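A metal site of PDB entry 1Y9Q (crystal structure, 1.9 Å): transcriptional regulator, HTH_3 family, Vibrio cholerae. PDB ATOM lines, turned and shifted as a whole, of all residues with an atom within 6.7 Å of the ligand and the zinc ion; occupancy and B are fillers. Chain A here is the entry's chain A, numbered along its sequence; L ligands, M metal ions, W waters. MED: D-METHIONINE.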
ATOM      1  N   ILE A  53     -10.483   9.715  11.626  1.00  0.00           N
ATOM      2  CA  ILE A  53     -11.933   9.808  11.688  1.00  0.00           C
ATOM      3  C   ILE A  53     -12.390  10.732  10.567  1.00  0.00           C
ATOM      4  O   ILE A  53     -13.423  10.494   9.945  1.00  0.00           O
ATOM      5  CB  ILE A  53     -12.384  10.396  13.047  1.00  0.00           C
ATOM      6  CG1 ILE A  53     -12.073   9.384  14.162  1.00  0.00           C
ATOM      7  CG2 ILE A  53     -13.876  10.728  13.004  1.00  0.00           C
ATOM      8  CD1 ILE A  53     -12.478   9.836  15.561  1.00  0.00           C
ATOM      9  N   ALA A  54     -11.615  11.775  10.293  1.00  0.00           N
ATOM     10  CA  ALA A  54     -11.979  12.721   9.251  1.00  0.00           C
ATOM     11  C   ALA A  54     -11.967  12.071   7.863  1.00  0.00           C
ATOM     12  O   ALA A  54     -12.823  12.369   7.023  1.00  0.00           O
ATOM     13  CB  ALA A  54     -11.042  13.925   9.277  1.00  0.00           C
ATOM     14  N   TRP A  57     -15.097   9.824   7.428  1.00  0.00           N
ATOM     15  CA  TRP A  57     -16.297  10.576   7.078  1.00  0.00           C
ATOM     16  C   TRP A  57     -16.237  11.002   5.616  1.00  0.00           C
ATOM     17  O   TRP A  57     -17.248  11.024   4.910  1.00  0.00           O
ATOM     18  CB  TRP A  57     -16.458  11.805   7.967  1.00  0.00           C
ATOM     19  CG  TRP A  57     -17.111  11.494   9.288  1.00  0.00           C
ATOM     20  CD1 TRP A  57     -16.482  11.208  10.468  1.00  0.00           C
ATOM     21  CD2 TRP A  57     -18.513  11.393   9.548  1.00  0.00           C
ATOM     22  NE1 TRP A  57     -17.414  10.938  11.439  1.00  0.00           N
ATOM     23  CE2 TRP A  57     -18.666  11.039  10.900  1.00  0.00           C
ATOM     24  CE3 TRP A  57     -19.654  11.569   8.754  1.00  0.00           C
ATOM     25  CZ2 TRP A  57     -19.925  10.849  11.486  1.00  0.00           C
ATOM     26  CZ3 TRP A  57     -20.906  11.382   9.337  1.00  0.00           C
ATOM     27  CH2 TRP A  57     -21.031  11.021  10.688  1.00  0.00           C
ATOM     28  N   PHE A  67     -21.605   6.578   8.826  1.00  0.00           N
ATOM     29  CA  PHE A  67     -20.328   6.313   9.480  1.00  0.00           C
ATOM     30  C   PHE A  67     -20.450   4.895  10.063  1.00  0.00           C
ATOM     31  O   PHE A  67     -19.506   4.104  10.041  1.00  0.00           O
ATOM     32  CB  PHE A  67     -20.100   7.339  10.603  1.00  0.00           C
ATOM     33  CG  PHE A  67     -18.805   7.169  11.348  1.00  0.00           C
ATOM     34  CD1 PHE A  67     -17.608   7.652  10.822  1.00  0.00           C
ATOM     35  CD2 PHE A  67     -18.776   6.532  12.595  1.00  0.00           C
ATOM     36  CE1 PHE A  67     -16.409   7.505  11.519  1.00  0.00           C
ATOM     37  CE2 PHE A  67     -17.576   6.391  13.300  1.00  0.00           C
ATOM     38  CZ  PHE A  67     -16.391   6.883  12.758  1.00  0.00           C
ATOM     39  N   MET A  90      -9.643  12.578  20.884  1.00  0.00           N
ATOM     40  CA  MET A  90     -11.065  12.571  20.574  1.00  0.00           C
ATOM     41  C   MET A  90     -11.574  11.146  20.749  1.00  0.00           C
ATOM     42  O   MET A  90     -11.046  10.218  20.157  1.00  0.00           O
ATOM     43  CB  MET A  90     -11.289  13.029  19.133  1.00  0.00           C
ATOM     44  CG  MET A  90     -12.743  13.020  18.692  1.00  0.00           C
ATOM     45  SD  MET A  90     -12.973  13.698  16.900  1.00  0.00           S
ATOM     46  CE  MET A  90     -14.124  15.195  17.287  1.00  0.00           C
ATOM     47  N   ILE A  92     -14.989   8.622  20.641  1.00  0.00           N
ATOM     48  CA  ILE A  92     -16.353   8.485  20.125  1.00  0.00           C
ATOM     49  C   ILE A  92     -17.147   7.399  20.851  1.00  0.00           C
ATOM     50  O   ILE A  92     -16.734   6.246  20.903  1.00  0.00           O
ATOM     51  CB  ILE A  92     -16.345   8.111  18.622  1.00  0.00           C
ATOM     52  CG1 ILE A  92     -15.382   9.008  17.850  1.00  0.00           C
ATOM     53  CG2 ILE A  92     -17.760   8.235  18.050  1.00  0.00           C
ATOM     54  CD1 ILE A  92     -15.685  10.467  17.941  1.00  0.00           C
ATOM     55  N   PHE A 107     -23.952  10.143  18.516  1.00  0.00           N
ATOM     56  CA  PHE A 107     -22.700   9.947  19.226  1.00  0.00           C
ATOM     57  C   PHE A 107     -22.531  10.882  20.415  1.00  0.00           C
ATOM     58  O   PHE A 107     -23.156  11.945  20.486  1.00  0.00           O
ATOM     59  CB  PHE A 107     -21.519  10.216  18.307  1.00  0.00           C
ATOM     60  CG  PHE A 107     -21.603   9.533  16.989  1.00  0.00           C
ATOM     61  CD1 PHE A 107     -21.191   8.217  16.833  1.00  0.00           C
ATOM     62  CD2 PHE A 107     -22.077  10.223  15.868  1.00  0.00           C
ATOM     63  CE1 PHE A 107     -21.245   7.590  15.593  1.00  0.00           C
ATOM     64  CE2 PHE A 107     -22.136   9.603  14.624  1.00  0.00           C
ATOM     65  CZ  PHE A 107     -21.715   8.291  14.489  1.00  0.00           C
ATOM     66  N   GLU A 108     -21.684  10.465  21.346  1.00  0.00           N
ATOM     67  CA  GLU A 108     -21.326  11.285  22.495  1.00  0.00           C
ATOM     68  C   GLU A 108     -19.826  11.423  22.288  1.00  0.00           C
ATOM     69  O   GLU A 108     -19.092  10.439  22.351  1.00  0.00           O
ATOM     70  CB  GLU A 108     -21.623  10.567  23.817  1.00  0.00           C
ATOM     71  CG  GLU A 108     -21.372  11.453  25.027  1.00  0.00           C
ATOM     72  CD  GLU A 108     -22.008  10.927  26.290  1.00  0.00           C
ATOM     73  OE1 GLU A 108     -23.247  10.817  26.346  1.00  0.00           O
ATOM     74  OE2 GLU A 108     -21.252  10.636  27.247  1.00  0.00           O
ATOM     75  N   ILE A 109     -19.371  12.644  22.023  1.00  0.00           N
ATOM     76  CA  ILE A 109     -17.963  12.910  21.728  1.00  0.00           C
ATOM     77  C   ILE A 109     -17.215  13.634  22.842  1.00  0.00           C
ATOM     78  O   ILE A 109     -17.688  14.636  23.370  1.00  0.00           O
ATOM     79  CB  ILE A 109     -17.830  13.784  20.461  1.00  0.00           C
ATOM     80  CG1 ILE A 109     -18.654  13.191  19.315  1.00  0.00           C
ATOM     81  CG2 ILE A 109     -16.364  13.912  20.067  1.00  0.00           C
ATOM     82  CD1 ILE A 109     -18.365  11.746  19.028  1.00  0.00           C
ATOM     83  N   GLN A 117     -10.980  19.657  15.700  1.00  0.00           N
ATOM     84  CA  GLN A 117     -11.307  18.696  14.650  1.00  0.00           C
ATOM     85  C   GLN A 117     -11.997  19.343  13.454  1.00  0.00           C
ATOM     86  O   GLN A 117     -13.140  19.777  13.554  1.00  0.00           O
ATOM     87  CB  GLN A 117     -12.231  17.621  15.256  1.00  0.00           C
ATOM     88  CG  GLN A 117     -12.616  16.484  14.336  1.00  0.00           C
ATOM     89  CD  GLN A 117     -11.452  15.571  14.030  1.00  0.00           C
ATOM     90  OE1 GLN A 117     -10.507  15.456  14.805  1.00  0.00           O
ATOM     91  NE2 GLN A 117     -11.514  14.908  12.882  1.00  0.00           N
ATOM     92  N   MET A 118     -11.283  19.455  12.330  1.00  0.00           N
ATOM     93  CA  MET A 118     -11.886  20.014  11.131  1.00  0.00           C
ATOM     94  C   MET A 118     -12.399  18.858  10.276  1.00  0.00           C
ATOM     95  O   MET A 118     -11.773  17.800  10.213  1.00  0.00           O
ATOM     96  CB  MET A 118     -10.877  20.832  10.332  1.00  0.00           C
ATOM     97  CG  MET A 118     -10.332  22.035  11.083  1.00  0.00           C
ATOM     98  SD  MET A 118     -11.718  23.136  11.836  1.00  0.00           S
ATOM     99  CE  MET A 118     -12.492  23.768  10.177  1.00  0.00           C
ATOM    100  N   SER A 119     -13.531  19.061   9.613  1.00  0.00           N
ATOM    101  CA  SER A 119     -14.131  18.017   8.780  1.00  0.00           C
ATOM    102  C   SER A 119     -14.418  18.487   7.369  1.00  0.00           C
ATOM    103  O   SER A 119     -14.629  19.670   7.128  1.00  0.00           O
ATOM    104  CB  SER A 119     -15.461  17.554   9.394  1.00  0.00           C
ATOM    105  OG  SER A 119     -15.285  17.006  10.672  1.00  0.00           O
ATOM    106  N   SER A 120     -14.427  17.533   6.438  1.00  0.00           N
ATOM    107  CA  SER A 120     -14.745  17.820   5.042  1.00  0.00           C
ATOM    108  C   SER A 120     -16.274  17.810   5.007  1.00  0.00           C
ATOM    109  O   SER A 120     -16.914  17.313   5.922  1.00  0.00           O
ATOM    110  CB  SER A 120     -14.213  16.727   4.116  1.00  0.00           C
ATOM    111  OG  SER A 120     -12.806  16.660   4.131  1.00  0.00           O
ATOM    112  N   HIS A 122     -19.982  16.717   4.668  1.00  0.00           N
ATOM    113  CA  HIS A 122     -20.587  15.382   4.696  1.00  0.00           C
ATOM    114  C   HIS A 122     -21.478  15.392   3.457  1.00  0.00           C
ATOM    115  O   HIS A 122     -21.509  16.391   2.737  1.00  0.00           O
ATOM    116  CB  HIS A 122     -21.405  15.172   5.976  1.00  0.00           C
ATOM    117  CG  HIS A 122     -20.577  15.172   7.220  1.00  0.00           C
ATOM    118  ND1 HIS A 122     -19.290  14.665   7.257  1.00  0.00           N
ATOM    119  CD2 HIS A 122     -20.852  15.597   8.474  1.00  0.00           C
ATOM    120  CE1 HIS A 122     -18.813  14.778   8.489  1.00  0.00           C
ATOM    121  NE2 HIS A 122     -19.733  15.336   9.246  1.00  0.00           N
ATOM    122  N   GLU A 128     -26.443  18.302  11.204  1.00  0.00           N
ATOM    123  CA  GLU A 128     -25.927  17.937  12.516  1.00  0.00           C
ATOM    124  C   GLU A 128     -26.509  18.769  13.632  1.00  0.00           C
ATOM    125  O   GLU A 128     -26.782  19.964  13.446  1.00  0.00           O
ATOM    126  CB  GLU A 128     -24.405  18.062  12.567  1.00  0.00           C
ATOM    127  CG  GLU A 128     -23.666  16.938  11.862  1.00  0.00           C
ATOM    128  CD  GLU A 128     -22.171  17.006  12.087  1.00  0.00           C
ATOM    129  OE1 GLU A 128     -21.747  17.201  13.243  1.00  0.00           O
ATOM    130  OE2 GLU A 128     -21.423  16.876  11.098  1.00  0.00           O
ATOM    131  N   PHE A 156     -26.724  22.670  12.300  1.00  0.00           N
ATOM    132  CA  PHE A 156     -26.213  23.277  11.078  1.00  0.00           C
ATOM    133  C   PHE A 156     -26.171  22.278   9.931  1.00  0.00           C
ATOM    134  O   PHE A 156     -26.202  21.066  10.154  1.00  0.00           O
ATOM    135  CB  PHE A 156     -24.804  23.833  11.325  1.00  0.00           C
ATOM    136  CG  PHE A 156     -23.786  22.776  11.674  1.00  0.00           C
ATOM    137  CD1 PHE A 156     -22.981  22.208  10.694  1.00  0.00           C
ATOM    138  CD2 PHE A 156     -23.633  22.361  12.996  1.00  0.00           C
ATOM    139  CE1 PHE A 156     -22.028  21.238  11.017  1.00  0.00           C
ATOM    140  CE2 PHE A 156     -22.696  21.383  13.328  1.00  0.00           C
ATOM    141  CZ  PHE A 156     -21.889  20.827  12.340  1.00  0.00           C
ATOM    142  N   SER A 158     -24.295  20.241   7.577  1.00  0.00           N
ATOM    143  CA  SER A 158     -22.938  19.727   7.581  1.00  0.00           C
ATOM    144  C   SER A 158     -22.328  19.414   6.225  1.00  0.00           C
ATOM    145  O   SER A 158     -21.188  18.941   6.154  1.00  0.00           O
ATOM    146  CB  SER A 158     -22.850  18.482   8.472  1.00  0.00           C
ATOM    147  OG  SER A 158     -23.575  17.392   7.913  1.00  0.00           O
ATOM    148  N   HIS A 162     -16.696  22.091   8.039  1.00  0.00           N
ATOM    149  CA  HIS A 162     -17.091  22.385   9.414  1.00  0.00           C
ATOM    150  C   HIS A 162     -16.053  21.854  10.378  1.00  0.00           C
ATOM    151  O   HIS A 162     -15.045  21.281   9.954  1.00  0.00           O
ATOM    152  CB  HIS A 162     -18.490  21.808   9.736  1.00  0.00           C
ATOM    153  CG  HIS A 162     -18.590  20.313   9.615  1.00  0.00           C
ATOM    154  ND1 HIS A 162     -18.592  19.662   8.407  1.00  0.00           N
ATOM    155  CD2 HIS A 162     -18.750  19.355  10.559  1.00  0.00           C
ATOM    156  CE1 HIS A 162     -18.754  18.364   8.608  1.00  0.00           C
ATOM    157  NE2 HIS A 162     -18.849  18.149   9.908  1.00  0.00           N
ATOM    158  N   GLY A 163     -16.278  22.048  11.667  1.00  0.00           N
ATOM    159  CA  GLY A 163     -15.308  21.564  12.634  1.00  0.00           C
ATOM    160  C   GLY A 163     -15.767  21.716  14.066  1.00  0.00           C
ATOM    161  O   GLY A 163     -16.782  22.356  14.328  1.00  0.00           O
ATOM    162  N   TYR A 164     -15.010  21.118  14.972  1.00  0.00           N
ATOM    163  CA  TYR A 164     -15.328  21.168  16.400  1.00  0.00           C
ATOM    164  C   TYR A 164     -14.036  21.411  17.167  1.00  0.00           C
ATOM    165  O   TYR A 164     -12.985  20.889  16.797  1.00  0.00           O
ATOM    166  CB  TYR A 164     -15.911  19.839  16.860  1.00  0.00           C
ATOM    167  CG  TYR A 164     -16.809  19.180  15.841  1.00  0.00           C
ATOM    168  CD1 TYR A 164     -16.275  18.504  14.745  1.00  0.00           C
ATOM    169  CD2 TYR A 164     -18.190  19.258  15.951  1.00  0.00           C
ATOM    170  CE1 TYR A 164     -17.089  17.916  13.783  1.00  0.00           C
ATOM    171  CE2 TYR A 164     -19.029  18.682  14.997  1.00  0.00           C
ATOM    172  CZ  TYR A 164     -18.464  18.011  13.917  1.00  0.00           C
ATOM    173  OH  TYR A 164     -19.291  17.457  12.983  1.00  0.00           O
ATOM    174  N   PHE A 173     -19.767  16.506  24.161  1.00  0.00           N
ATOM    175  CA  PHE A 173     -21.009  16.935  23.529  1.00  0.00           C
ATOM    176  C   PHE A 173     -21.709  15.814  22.787  1.00  0.00           C
ATOM    177  O   PHE A 173     -21.073  14.869  22.335  1.00  0.00           O
ATOM    178  CB  PHE A 173     -20.738  18.103  22.558  1.00  0.00           C
ATOM    179  CG  PHE A 173     -19.853  17.745  21.382  1.00  0.00           C
ATOM    180  CD1 PHE A 173     -20.409  17.467  20.138  1.00  0.00           C
ATOM    181  CD2 PHE A 173     -18.468  17.730  21.514  1.00  0.00           C
ATOM    182  CE1 PHE A 173     -19.605  17.187  19.034  1.00  0.00           C
ATOM    183  CE2 PHE A 173     -17.653  17.435  20.419  1.00  0.00           C
ATOM    184  CZ  PHE A 173     -18.227  17.174  19.179  1.00  0.00           C
ATOM    185  N   ASN A 175     -23.658  14.506  19.587  1.00  0.00           N
ATOM    186  CA  ASN A 175     -23.708  14.868  18.183  1.00  0.00           C
ATOM    187  C   ASN A 175     -24.722  13.971  17.477  1.00  0.00           C
ATOM    188  O   ASN A 175     -24.552  12.757  17.434  1.00  0.00           O
ATOM    189  CB  ASN A 175     -22.317  14.719  17.556  1.00  0.00           C
ATOM    190  CG  ASN A 175     -22.271  15.119  16.090  1.00  0.00           C
ATOM    191  OD1 ASN A 175     -22.949  16.056  15.660  1.00  0.00           O
ATOM    192  ND2 ASN A 175     -21.446  14.423  15.315  1.00  0.00           N
ATOM    193  N   VAL A 177     -26.309  13.070  13.928  1.00  0.00           N
ATOM    194  CA  VAL A 177     -26.068  13.260  12.490  1.00  0.00           C
ATOM    195  C   VAL A 177     -27.300  12.710  11.761  1.00  0.00           C
ATOM    196  O   VAL A 177     -27.577  11.513  11.809  1.00  0.00           O
ATOM    197  CB  VAL A 177     -24.800  12.506  12.034  1.00  0.00           C
ATOM    198  CG1 VAL A 177     -24.576  12.722  10.542  1.00  0.00           C
ATOM    199  CG2 VAL A 177     -23.593  12.986  12.819  1.00  0.00           C
HETATM  200  N   MED L   1     -19.835  14.545  12.324  1.00  0.00           N
HETATM  201  CA  MED L   1     -18.541  13.933  12.741  1.00  0.00           C
HETATM  202  C   MED L   1     -17.361  14.667  12.096  1.00  0.00           C
HETATM  203  O   MED L   1     -17.502  15.638  11.330  1.00  0.00           O
HETATM  204  CB  MED L   1     -18.453  13.962  14.291  1.00  0.00           C
HETATM  205  CG  MED L   1     -17.243  13.376  14.982  1.00  0.00           C
HETATM  206  SD  MED L   1     -17.314  11.581  14.687  1.00  0.00           S
HETATM  207  CE  MED L   1     -18.772  11.117  15.516  1.00  0.00           C
HETATM  208  OXT MED L   1     -16.207  14.285  12.332  1.00  0.00           O
HETATM  209 ZN    ZN M   1     -19.443  16.339  11.080  1.00  0.00          ZN
HETATM  210  O   HOH W   1     -15.106  14.370   9.612  1.00  0.00           O
HETATM  211  O   HOH W   2     -13.817  15.223  11.567  1.00  0.00           O
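A sulfur (SD) of the ligand lies close to the indole nitrogen (NE1) of Trp 57 (3.3 Å).
An oxygen (OXT) of the ligand is in hydrogen-bond range of the side-chain hydroxyl of Ser 119, 3.3 Å away.
N of the ligand sits close to ND2 of Asn 175 (3.4 Å).
The backbone carbonyl oxygen (O) of Tyr 164 lies within hydrogen-bond range of the backbone NH (N) of Gln 117, 2.6 Å away.
The backbone NH (N) of Ile 109 lies within hydrogen-bond range of the backbone carbonyl oxygen (O) of Phe 173 (2.8 Å).
O of His 162 sits at hydrogen-bond distance from N of Ser 119.
N of Phe 156 sits at hydrogen-bond distance from O of Glu 128 (2.9 Å).
N of Asn 175 is in hydrogen-bond range of O of Phe 107, 2.8 Å away.
The side-chain carboxylate (OE1) of Glu 128 sits close to the side-chain amide oxygen (OD1) of Asn 175.
The backbone NH (N) of His 122 is in hydrogen-bond range of the backbone carbonyl oxygen (O) of Ser 158.
Ile 53 touches the ligand.
Ile 92 touches the ligand (CD1 to SD, 3.8 Å).
CD2 of Phe 107 touches CE of the ligand, at 3.4 Å.
Ile 109 touches the ligand.
11 residues have an atom within 4 Å of the ligand: Ile 53, Trp 57, Ile 92, Phe 107, Ile 109, Ser 119, His 122, Glu 128, His 162, Tyr 164 and Asn 175.
Along chain A the residues within 4 Å of the ligand span positions 53 to 175.
Of the 23 residues printed, 4 come within 4 Å of the zinc ion.
Along chain A the residues within 4 Å of the zinc ion span positions 122 to 164.
The nearest printed residue that does not touch the zinc ion is Ser 119 (4.2 Å).
The zinc ion is bound by OE2 of Glu 128 (2.1 Å), O of the ligand (2.1 Å), NE2 of His 122 (2.1 Å), OH of Tyr 164 (2.2 Å), N of the ligand (2.2 Å) and NE2 of His 162 (2.2 Å).
Water W2 lies within hydrogen-bond range of the side-chain hydroxyl (OG) of Ser 119 (2.5 Å), the side-chain amide nitrogen (NE2) of Gln 117 (2.7 Å) and an oxygen (OXT) of the ligand (2.7 Å).
Water W1 bridges OG of Ser 119 (2.8 Å) and OXT of the ligand (2.9 Å).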
